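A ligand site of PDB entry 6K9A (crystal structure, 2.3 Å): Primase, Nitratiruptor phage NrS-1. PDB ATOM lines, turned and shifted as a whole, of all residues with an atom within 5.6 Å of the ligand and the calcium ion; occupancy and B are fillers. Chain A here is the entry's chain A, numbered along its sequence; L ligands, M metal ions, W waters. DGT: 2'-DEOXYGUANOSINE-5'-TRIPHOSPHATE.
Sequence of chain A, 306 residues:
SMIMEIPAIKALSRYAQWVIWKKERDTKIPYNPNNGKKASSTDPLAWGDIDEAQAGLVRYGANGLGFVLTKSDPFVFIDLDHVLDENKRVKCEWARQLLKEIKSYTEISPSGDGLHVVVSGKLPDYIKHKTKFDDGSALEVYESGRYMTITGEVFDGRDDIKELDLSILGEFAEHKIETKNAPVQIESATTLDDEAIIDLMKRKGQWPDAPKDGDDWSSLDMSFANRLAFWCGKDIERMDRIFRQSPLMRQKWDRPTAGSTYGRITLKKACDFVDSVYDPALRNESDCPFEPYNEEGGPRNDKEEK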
ATOM      1  N   ASP A  26     -19.693  16.379 -32.548  1.00  0.00           N
ATOM      2  CA  ASP A  26     -21.091  16.410 -32.151  1.00  0.00           C
ATOM      3  C   ASP A  26     -21.594  15.048 -31.682  1.00  0.00           C
ATOM      4  O   ASP A  26     -22.787  14.924 -31.347  1.00  0.00           O
ATOM      5  CB  ASP A  26     -21.968  16.900 -33.308  1.00  0.00           C
ATOM      6  CG  ASP A  26     -21.772  18.379 -33.583  1.00  0.00           C
ATOM      7  OD1 ASP A  26     -21.346  19.110 -32.660  1.00  0.00           O
ATOM      8  OD2 ASP A  26     -22.045  18.810 -34.726  1.00  0.00           O
ATOM      9  N   THR A  27     -20.738  14.035 -31.641  1.00  0.00           N
ATOM     10  CA  THR A  27     -21.120  12.702 -31.215  1.00  0.00           C
ATOM     11  C   THR A  27     -20.791  12.503 -29.732  1.00  0.00           C
ATOM     12  O   THR A  27     -19.994  13.223 -29.142  1.00  0.00           O
ATOM     13  CB  THR A  27     -20.409  11.629 -32.039  1.00  0.00           C
ATOM     14  OG1 THR A  27     -19.003  11.694 -31.811  1.00  0.00           O
ATOM     15  CG2 THR A  27     -20.686  11.829 -33.520  1.00  0.00           C
ATOM     16  N   LYS A  28     -21.446  11.506 -29.145  1.00  0.00           N
ATOM     17  CA  LYS A  28     -21.235  11.123 -27.747  1.00  0.00           C
ATOM     18  C   LYS A  28     -20.944   9.626 -27.737  1.00  0.00           C
ATOM     19  O   LYS A  28     -21.858   8.805 -27.820  1.00  0.00           O
ATOM     20  CB  LYS A  28     -22.453  11.479 -26.891  1.00  0.00           C
ATOM     21  CG  LYS A  28     -22.857  12.943 -26.960  1.00  0.00           C
ATOM     22  CD  LYS A  28     -24.065  13.235 -26.099  1.00  0.00           C
ATOM     23  CE  LYS A  28     -24.465  14.699 -26.181  1.00  0.00           C
ATOM     24  NZ  LYS A  28     -24.890  15.068 -27.567  1.00  0.00           N
ATOM     25  N   ILE A  29     -19.667   9.281 -27.621  1.00  0.00           N
ATOM     26  CA  ILE A  29     -19.217   7.896 -27.778  1.00  0.00           C
ATOM     27  C   ILE A  29     -19.321   7.159 -26.451  1.00  0.00           C
ATOM     28  O   ILE A  29     -18.808   7.640 -25.433  1.00  0.00           O
ATOM     29  CB  ILE A  29     -17.778   7.838 -28.324  1.00  0.00           C
ATOM     30  CG1 ILE A  29     -17.695   8.533 -29.686  1.00  0.00           C
ATOM     31  CG2 ILE A  29     -17.293   6.398 -28.415  1.00  0.00           C
ATOM     32  CD1 ILE A  29     -18.708   8.028 -30.674  1.00  0.00           C
ATOM     33  N   PRO A  30     -19.968   6.000 -26.415  1.00  0.00           N
ATOM     34  CA  PRO A  30     -20.051   5.231 -25.163  1.00  0.00           C
ATOM     35  C   PRO A  30     -18.732   4.548 -24.830  1.00  0.00           C
ATOM     36  O   PRO A  30     -17.968   4.149 -25.715  1.00  0.00           O
ATOM     37  CB  PRO A  30     -21.145   4.193 -25.462  1.00  0.00           C
ATOM     38  CG  PRO A  30     -21.116   4.034 -26.944  1.00  0.00           C
ATOM     39  CD  PRO A  30     -20.747   5.385 -27.501  1.00  0.00           C
ATOM     40  N   SER A  41     -22.646  -1.423 -28.029  1.00  0.00           N
ATOM     41  CA  SER A  41     -24.015  -1.256 -27.560  1.00  0.00           C
ATOM     42  C   SER A  41     -24.792  -2.562 -27.532  1.00  0.00           C
ATOM     43  O   SER A  41     -25.940  -2.572 -27.082  1.00  0.00           O
ATOM     44  CB  SER A  41     -24.749  -0.228 -28.424  1.00  0.00           C
ATOM     45  OG  SER A  41     -24.197   1.069 -28.250  1.00  0.00           O
ATOM     46  N   PHE A  77     -36.920   4.743 -25.026  1.00  0.00           N
ATOM     47  CA  PHE A  77     -36.209   6.020 -25.022  1.00  0.00           C
ATOM     48  C   PHE A  77     -36.836   6.933 -26.072  1.00  0.00           C
ATOM     49  O   PHE A  77     -36.824   6.617 -27.265  1.00  0.00           O
ATOM     50  CB  PHE A  77     -34.719   5.792 -25.302  1.00  0.00           C
ATOM     51  CG  PHE A  77     -33.931   7.056 -25.555  1.00  0.00           C
ATOM     52  CD1 PHE A  77     -32.900   7.053 -26.490  1.00  0.00           C
ATOM     53  CD2 PHE A  77     -34.219   8.229 -24.879  1.00  0.00           C
ATOM     54  CE1 PHE A  77     -32.172   8.201 -26.723  1.00  0.00           C
ATOM     55  CE2 PHE A  77     -33.500   9.376 -25.122  1.00  0.00           C
ATOM     56  CZ  PHE A  77     -32.467   9.368 -26.048  1.00  0.00           C
ATOM     57  N   ASP A  79     -36.545  10.694 -27.615  1.00  0.00           N
ATOM     58  CA  ASP A  79     -35.587  11.798 -27.719  1.00  0.00           C
ATOM     59  C   ASP A  79     -36.223  12.935 -28.496  1.00  0.00           C
ATOM     60  O   ASP A  79     -36.624  12.763 -29.649  1.00  0.00           O
ATOM     61  CB  ASP A  79     -34.286  11.329 -28.389  1.00  0.00           C
ATOM     62  CG  ASP A  79     -33.179  12.356 -28.271  1.00  0.00           C
ATOM     63  OD1 ASP A  79     -33.270  13.233 -27.395  1.00  0.00           O
ATOM     64  OD2 ASP A  79     -32.218  12.270 -29.063  1.00  0.00           O
ATOM     65  N   LEU A  80     -36.289  14.110 -27.865  1.00  0.00           N
ATOM     66  CA  LEU A  80     -36.853  15.317 -28.463  1.00  0.00           C
ATOM     67  C   LEU A  80     -35.714  16.299 -28.676  1.00  0.00           C
ATOM     68  O   LEU A  80     -35.201  16.889 -27.720  1.00  0.00           O
ATOM     69  CB  LEU A  80     -37.944  15.919 -27.580  1.00  0.00           C
ATOM     70  CG  LEU A  80     -39.250  15.137 -27.331  1.00  0.00           C
ATOM     71  CD1 LEU A  80     -39.055  13.964 -26.385  1.00  0.00           C
ATOM     72  CD2 LEU A  80     -40.319  16.068 -26.806  1.00  0.00           C
ATOM     73  N   ASP A  81     -35.316  16.484 -29.935  1.00  0.00           N
ATOM     74  CA  ASP A  81     -34.173  17.323 -30.269  1.00  0.00           C
ATOM     75  C   ASP A  81     -34.613  18.771 -30.476  1.00  0.00           C
ATOM     76  O   ASP A  81     -35.612  19.032 -31.161  1.00  0.00           O
ATOM     77  CB  ASP A  81     -33.465  16.825 -31.527  1.00  0.00           C
ATOM     78  CG  ASP A  81     -32.741  15.509 -31.305  1.00  0.00           C
ATOM     79  OD1 ASP A  81     -32.443  15.189 -30.141  1.00  0.00           O
ATOM     80  OD2 ASP A  81     -32.453  14.810 -32.300  1.00  0.00           O
ATOM     81  N   SER A 109     -31.566  17.121 -21.981  1.00  0.00           N
ATOM     82  CA  SER A 109     -30.430  16.438 -22.587  1.00  0.00           C
ATOM     83  C   SER A 109     -29.171  17.290 -22.436  1.00  0.00           C
ATOM     84  O   SER A 109     -29.242  18.472 -22.106  1.00  0.00           O
ATOM     85  CB  SER A 109     -30.743  16.141 -24.051  1.00  0.00           C
ATOM     86  OG  SER A 109     -30.967  17.338 -24.790  1.00  0.00           O
ATOM     87  N   PRO A 110     -27.983  16.689 -22.656  1.00  0.00           N
ATOM     88  CA  PRO A 110     -26.730  17.412 -22.370  1.00  0.00           C
ATOM     89  C   PRO A 110     -26.581  18.773 -23.044  1.00  0.00           C
ATOM     90  O   PRO A 110     -26.019  19.687 -22.431  1.00  0.00           O
ATOM     91  CB  PRO A 110     -25.659  16.431 -22.855  1.00  0.00           C
ATOM     92  CG  PRO A 110     -26.258  15.106 -22.634  1.00  0.00           C
ATOM     93  CD  PRO A 110     -27.724  15.263 -22.933  1.00  0.00           C
ATOM     94  N   SER A 111     -27.058  18.932 -24.276  1.00  0.00           N
ATOM     95  CA  SER A 111     -26.914  20.230 -24.943  1.00  0.00           C
ATOM     96  C   SER A 111     -27.787  21.310 -24.336  1.00  0.00           C
ATOM     97  O   SER A 111     -27.568  22.495 -24.618  1.00  0.00           O
ATOM     98  CB  SER A 111     -27.221  20.105 -26.439  1.00  0.00           C
ATOM     99  OG  SER A 111     -26.260  19.296 -27.092  1.00  0.00           O
ATOM    100  N   GLY A 112     -28.763  20.947 -23.500  1.00  0.00           N
ATOM    101  CA  GLY A 112     -29.605  21.909 -22.820  1.00  0.00           C
ATOM    102  C   GLY A 112     -30.832  22.361 -23.584  1.00  0.00           C
ATOM    103  O   GLY A 112     -31.689  23.025 -22.990  1.00  0.00           O
ATOM    104  N   ASP A 113     -30.932  22.022 -24.866  1.00  0.00           N
ATOM    105  CA  ASP A 113     -32.051  22.461 -25.698  1.00  0.00           C
ATOM    106  C   ASP A 113     -32.983  21.318 -26.091  1.00  0.00           C
ATOM    107  O   ASP A 113     -33.885  21.519 -26.898  1.00  0.00           O
ATOM    108  CB  ASP A 113     -31.535  23.161 -26.956  1.00  0.00           C
ATOM    109  CG  ASP A 113     -30.830  22.211 -27.904  1.00  0.00           C
ATOM    110  OD1 ASP A 113     -30.141  21.291 -27.422  1.00  0.00           O
ATOM    111  OD2 ASP A 113     -30.980  22.381 -29.127  1.00  0.00           O
ATOM    112  N   GLY A 114     -32.782  20.121 -25.530  1.00  0.00           N
ATOM    113  CA  GLY A 114     -33.605  18.976 -25.849  1.00  0.00           C
ATOM    114  C   GLY A 114     -34.057  18.247 -24.600  1.00  0.00           C
ATOM    115  O   GLY A 114     -33.687  18.603 -23.476  1.00  0.00           O
ATOM    116  N   LEU A 115     -34.868  17.216 -24.822  1.00  0.00           N
ATOM    117  CA  LEU A 115     -35.464  16.451 -23.738  1.00  0.00           C
ATOM    118  C   LEU A 115     -35.317  14.960 -23.998  1.00  0.00           C
ATOM    119  O   LEU A 115     -35.206  14.513 -25.140  1.00  0.00           O
ATOM    120  CB  LEU A 115     -36.955  16.791 -23.566  1.00  0.00           C
ATOM    121  CG  LEU A 115     -37.287  18.199 -23.089  1.00  0.00           C
ATOM    122  CD1 LEU A 115     -38.780  18.402 -23.033  1.00  0.00           C
ATOM    123  CD2 LEU A 115     -36.656  18.463 -21.728  1.00  0.00           C
ATOM    124  N   HIS A 116     -35.310  14.205 -22.903  1.00  0.00           N
ATOM    125  CA  HIS A 116     -35.406  12.752 -22.938  1.00  0.00           C
ATOM    126  C   HIS A 116     -36.643  12.318 -22.177  1.00  0.00           C
ATOM    127  O   HIS A 116     -36.918  12.829 -21.091  1.00  0.00           O
ATOM    128  CB  HIS A 116     -34.165  12.093 -22.327  1.00  0.00           C
ATOM    129  CG  HIS A 116     -32.954  12.153 -23.197  1.00  0.00           C
ATOM    130  ND1 HIS A 116     -31.742  11.620 -22.815  1.00  0.00           N
ATOM    131  CD2 HIS A 116     -32.763  12.676 -24.430  1.00  0.00           C
ATOM    132  CE1 HIS A 116     -30.854  11.810 -23.772  1.00  0.00           C
ATOM    133  NE2 HIS A 116     -31.452  12.449 -24.768  1.00  0.00           N
ATOM    134  N   GLU A 140     -36.875  11.254 -31.974  1.00  0.00           N
ATOM    135  CA  GLU A 140     -36.240   9.964 -32.169  1.00  0.00           C
ATOM    136  C   GLU A 140     -36.653   9.018 -31.050  1.00  0.00           C
ATOM    137  O   GLU A 140     -36.596   9.387 -29.873  1.00  0.00           O
ATOM    138  CB  GLU A 140     -34.713  10.102 -32.224  1.00  0.00           C
ATOM    139  CG  GLU A 140     -34.073   9.392 -33.401  1.00  0.00           C
ATOM    140  CD  GLU A 140     -32.567   9.616 -33.480  1.00  0.00           C
ATOM    141  OE1 GLU A 140     -32.093  10.635 -32.936  1.00  0.00           O
ATOM    142  OE2 GLU A 140     -31.874   8.775 -34.070  1.00  0.00           O
ATOM    143  N   ARG A 146     -29.373   0.732 -28.894  1.00  0.00           N
ATOM    144  CA  ARG A 146     -28.746   2.015 -28.673  1.00  0.00           C
ATOM    145  C   ARG A 146     -28.717   2.475 -27.210  1.00  0.00           C
ATOM    146  O   ARG A 146     -29.470   1.992 -26.416  1.00  0.00           O
ATOM    147  CB  ARG A 146     -29.430   3.014 -29.580  1.00  0.00           C
ATOM    148  CG  ARG A 146     -30.094   4.169 -28.907  1.00  0.00           C
ATOM    149  CD  ARG A 146     -29.694   5.446 -29.630  1.00  0.00           C
ATOM    150  NE  ARG A 146     -29.950   5.377 -31.052  1.00  0.00           N
ATOM    151  CZ  ARG A 146     -29.426   6.182 -31.960  1.00  0.00           C
ATOM    152  NH1 ARG A 146     -28.573   7.126 -31.610  1.00  0.00           N
ATOM    153  NH2 ARG A 146     -29.740   6.007 -33.219  1.00  0.00           N
ATOM    154  N   TYR A 147     -27.790   3.339 -26.856  1.00  0.00           N
ATOM    155  CA  TYR A 147     -27.741   3.865 -25.500  1.00  0.00           C
ATOM    156  C   TYR A 147     -28.238   5.308 -25.465  1.00  0.00           C
ATOM    157  O   TYR A 147     -28.388   5.970 -26.493  1.00  0.00           O
ATOM    158  CB  TYR A 147     -26.313   3.786 -24.933  1.00  0.00           C
ATOM    159  CG  TYR A 147     -25.480   5.029 -25.112  1.00  0.00           C
ATOM    160  CD1 TYR A 147     -24.834   5.294 -26.322  1.00  0.00           C
ATOM    161  CD2 TYR A 147     -25.322   5.945 -24.081  1.00  0.00           C
ATOM    162  CE1 TYR A 147     -24.069   6.434 -26.483  1.00  0.00           C
ATOM    163  CE2 TYR A 147     -24.563   7.090 -24.236  1.00  0.00           C
ATOM    164  CZ  TYR A 147     -23.937   7.326 -25.437  1.00  0.00           C
ATOM    165  OH  TYR A 147     -23.173   8.453 -25.606  1.00  0.00           O
ATOM    166  N   MET A 148     -28.564   5.747 -24.281  1.00  0.00           N
ATOM    167  CA  MET A 148     -29.014   7.077 -24.027  1.00  0.00           C
ATOM    168  C   MET A 148     -28.217   7.797 -22.923  1.00  0.00           C
ATOM    169  O   MET A 148     -27.963   7.210 -21.915  1.00  0.00           O
ATOM    170  CB  MET A 148     -30.497   7.058 -23.693  1.00  0.00           C
ATOM    171  CG  MET A 148     -30.813   6.480 -22.337  1.00  0.00           C
ATOM    172  SD  MET A 148     -32.446   6.627 -21.640  1.00  0.00           S
ATOM    173  CE  MET A 148     -33.239   5.583 -22.742  1.00  0.00           C
ATOM    174  N   THR A 149     -27.865   9.061 -23.118  1.00  0.00           N
ATOM    175  CA  THR A 149     -27.207   9.806 -22.052  1.00  0.00           C
ATOM    176  C   THR A 149     -28.171  10.003 -20.893  1.00  0.00           C
ATOM    177  O   THR A 149     -29.395  10.086 -21.073  1.00  0.00           O
ATOM    178  CB  THR A 149     -26.720  11.155 -22.563  1.00  0.00           C
ATOM    179  OG1 THR A 149     -27.821  11.905 -23.094  1.00  0.00           O
ATOM    180  CG2 THR A 149     -25.677  10.968 -23.661  1.00  0.00           C
HETATM  181  PG  DGT L   1     -28.391  16.464 -27.145  1.00  0.00           P
HETATM  182  O1G DGT L   1     -27.212  17.024 -27.906  1.00  0.00           O
HETATM  183  O2G DGT L   1     -29.485  16.085 -28.103  1.00  0.00           O
HETATM  184  O3G DGT L   1     -28.906  17.498 -26.181  1.00  0.00           O
HETATM  185  O3B DGT L   1     -27.909  15.170 -26.318  1.00  0.00           O
HETATM  186  PB  DGT L   1     -28.305  13.649 -26.688  1.00  0.00           P
HETATM  187  O1B DGT L   1     -27.749  12.776 -25.596  1.00  0.00           O
HETATM  188  O2B DGT L   1     -29.802  13.460 -26.771  1.00  0.00           O
HETATM  189  O3A DGT L   1     -27.554  13.315 -28.078  1.00  0.00           O
HETATM  190  PA  DGT L   1     -28.292  12.950 -29.470  1.00  0.00           P
HETATM  191  O1A DGT L   1     -29.691  13.515 -29.535  1.00  0.00           O
HETATM  192  O2A DGT L   1     -27.477  13.462 -30.625  1.00  0.00           O
HETATM  193  O5' DGT L   1     -28.356  11.335 -29.535  1.00  0.00           O
HETATM  194  C5' DGT L   1     -29.321  10.592 -28.833  1.00  0.00           C
HETATM  195  C4' DGT L   1     -28.623   9.467 -28.075  1.00  0.00           C
HETATM  196  O4' DGT L   1     -27.849   8.687 -28.960  1.00  0.00           O
HETATM  197  C3' DGT L   1     -27.644   9.997 -27.039  1.00  0.00           C
HETATM  198  O3' DGT L   1     -28.260  10.104 -25.770  1.00  0.00           O
HETATM  199  C2' DGT L   1     -26.534   8.970 -27.026  1.00  0.00           C
HETATM  200  C1' DGT L   1     -26.648   8.248 -28.353  1.00  0.00           C
HETATM  201  N9  DGT L   1     -25.496   8.620 -29.185  1.00  0.00           N
HETATM  202  C8  DGT L   1     -25.152   9.896 -29.555  1.00  0.00           C
HETATM  203  N7  DGT L   1     -24.041   9.842 -30.321  1.00  0.00           N
HETATM  204  C5  DGT L   1     -23.656   8.556 -30.434  1.00  0.00           C
HETATM  205  C6  DGT L   1     -22.592   7.956 -31.103  1.00  0.00           C
HETATM  206  O6  DGT L   1     -21.797   8.653 -31.726  1.00  0.00           O
HETATM  207  N1  DGT L   1     -22.440   6.591 -31.060  1.00  0.00           N
HETATM  208  C2  DGT L   1     -23.348   5.825 -30.361  1.00  0.00           C
HETATM  209  N2  DGT L   1     -23.203   4.500 -30.313  1.00  0.00           N
HETATM  210  N3  DGT L   1     -24.406   6.419 -29.697  1.00  0.00           N
HETATM  211  C4  DGT L   1     -24.564   7.773 -29.734  1.00  0.00           C
HETATM  212 CA    CA M   1     -31.294  14.532 -28.213  1.00  0.00          CA
HETATM  213  O   HOH W   1     -28.043  18.818 -29.642  1.00  0.00           O
HETATM  214  O   HOH W   2     -24.858  13.727 -29.670  1.00  0.00           O
HETATM  215  O   HOH W   3     -29.184  16.857 -30.892  1.00  0.00           O
HETATM  216  O   HOH W   4     -31.685  18.726 -28.377  1.00  0.00           O
HETATM  217  O   HOH W   5     -32.521  15.941 -26.771  1.00  0.00           O
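The side-chain hydroxyl of Ser 109 lies within hydrogen-bond range of an oxygen (O3G) of the ligand (2.5 Å).
O3G of the ligand lies within hydrogen-bond range of N of Ser 111 (3.0 Å).
O1G of the ligand lies within hydrogen-bond range of OG of Ser 111.
An oxygen (O3') of the ligand lies within hydrogen-bond range of the backbone NH (N) of Thr 149, at 2.9 Å.
OG1 of Thr 149 is in hydrogen-bond range of O1B of the ligand (2.7 Å).
NE2 of His 116 sits close to O2B of the ligand, at 2.8 Å.
A nitrogen (N7) of the ligand lies within hydrogen-bond range of the backbone NH (N) of Lys 28, 3.3 Å away.
An oxygen (O1G) of the ligand lies within salt-bridge range of the side-chain amino group (NZ) of Lys 28 (3.1 Å).
The guanidinium group (NH1) of Arg 146 is in hydrogen-bond range of an oxygen (O4') of the ligand.
N of Ser 109 lies within hydrogen-bond range of O of Gly 114 (3.0 Å).
OD1 of Asp 79 lies close to NE2 of His 116, at 3.3 Å.
The backbone NH (N) of Asp 79 is in hydrogen-bond range of the backbone carbonyl oxygen (O) of Glu 140.
A ring nitrogen (ND1) of His 116 sits at hydrogen-bond distance from the backbone carbonyl oxygen (O) of Thr 149.
O of Lys 28 lies within hydrogen-bond range of OH of Tyr 147 (2.6 Å).
NH2 of Arg 146 lies within salt-bridge range of OE2 of Glu 140 (3.6 Å).
Thr 27 touches the ligand (CB to O6, 3.3 Å).
CD1 of Ile 29 touches O6 of the ligand, at 3.3 Å.
CD of Pro 30 touches N2 of the ligand (3.8 Å).
Pro 110 touches the ligand (CD to O3B, 3.4 Å).
Tyr 147 touches the ligand (CE1 to N3, 3.2 Å).
Met 148 touches the ligand (CA to O3', 3.6 Å).
Within 4 Å of the ligand: Thr 27, Lys 28, Ile 29, Pro 30, Asp 79, Asp 81, Ser 109, Pro 110, Ser 111, His 116, Arg 146, Tyr 147, Met 148 and Thr 149.
The nearest printed residue that does not touch the ligand is Phe 77 (4.003 Å).
Within 4 Å of the calcium ion: Asp 79 and Asp 81.
The calcium ion is bound by O1A of the ligand (2.3 Å), O2B of the ligand (2.3 Å), OD1 of Asp 81 (2.3 Å), water W5 (2.4 Å), O2G of the ligand (2.4 Å), OD1 of Asp 79 (2.5 Å) and OD2 of Asp 79 (2.6 Å).
The calcium ion has seven donor atoms within binding distance.
Water W5 lies within hydrogen-bond range of the side-chain hydroxyl of Ser 109 (2.9 Å), the backbone carbonyl oxygen of Leu 80 (3.0 Å) and the backbone NH of Leu 115 (3.3 Å).
Water W1 lies within hydrogen-bond range of O1G of the ligand (2.6 Å) and OG of Ser 111 (3.1 Å).
Water W2 lies within hydrogen-bond range of NZ of Lys 28 (2.5 Å), O2A of the ligand (2.8 Å) and O of Asp 26 (2.9 Å).
Water W4 lies within hydrogen-bond range of OD1 of Asp 113 (3.1 Å) and N of Gly 114 (3.4 Å).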
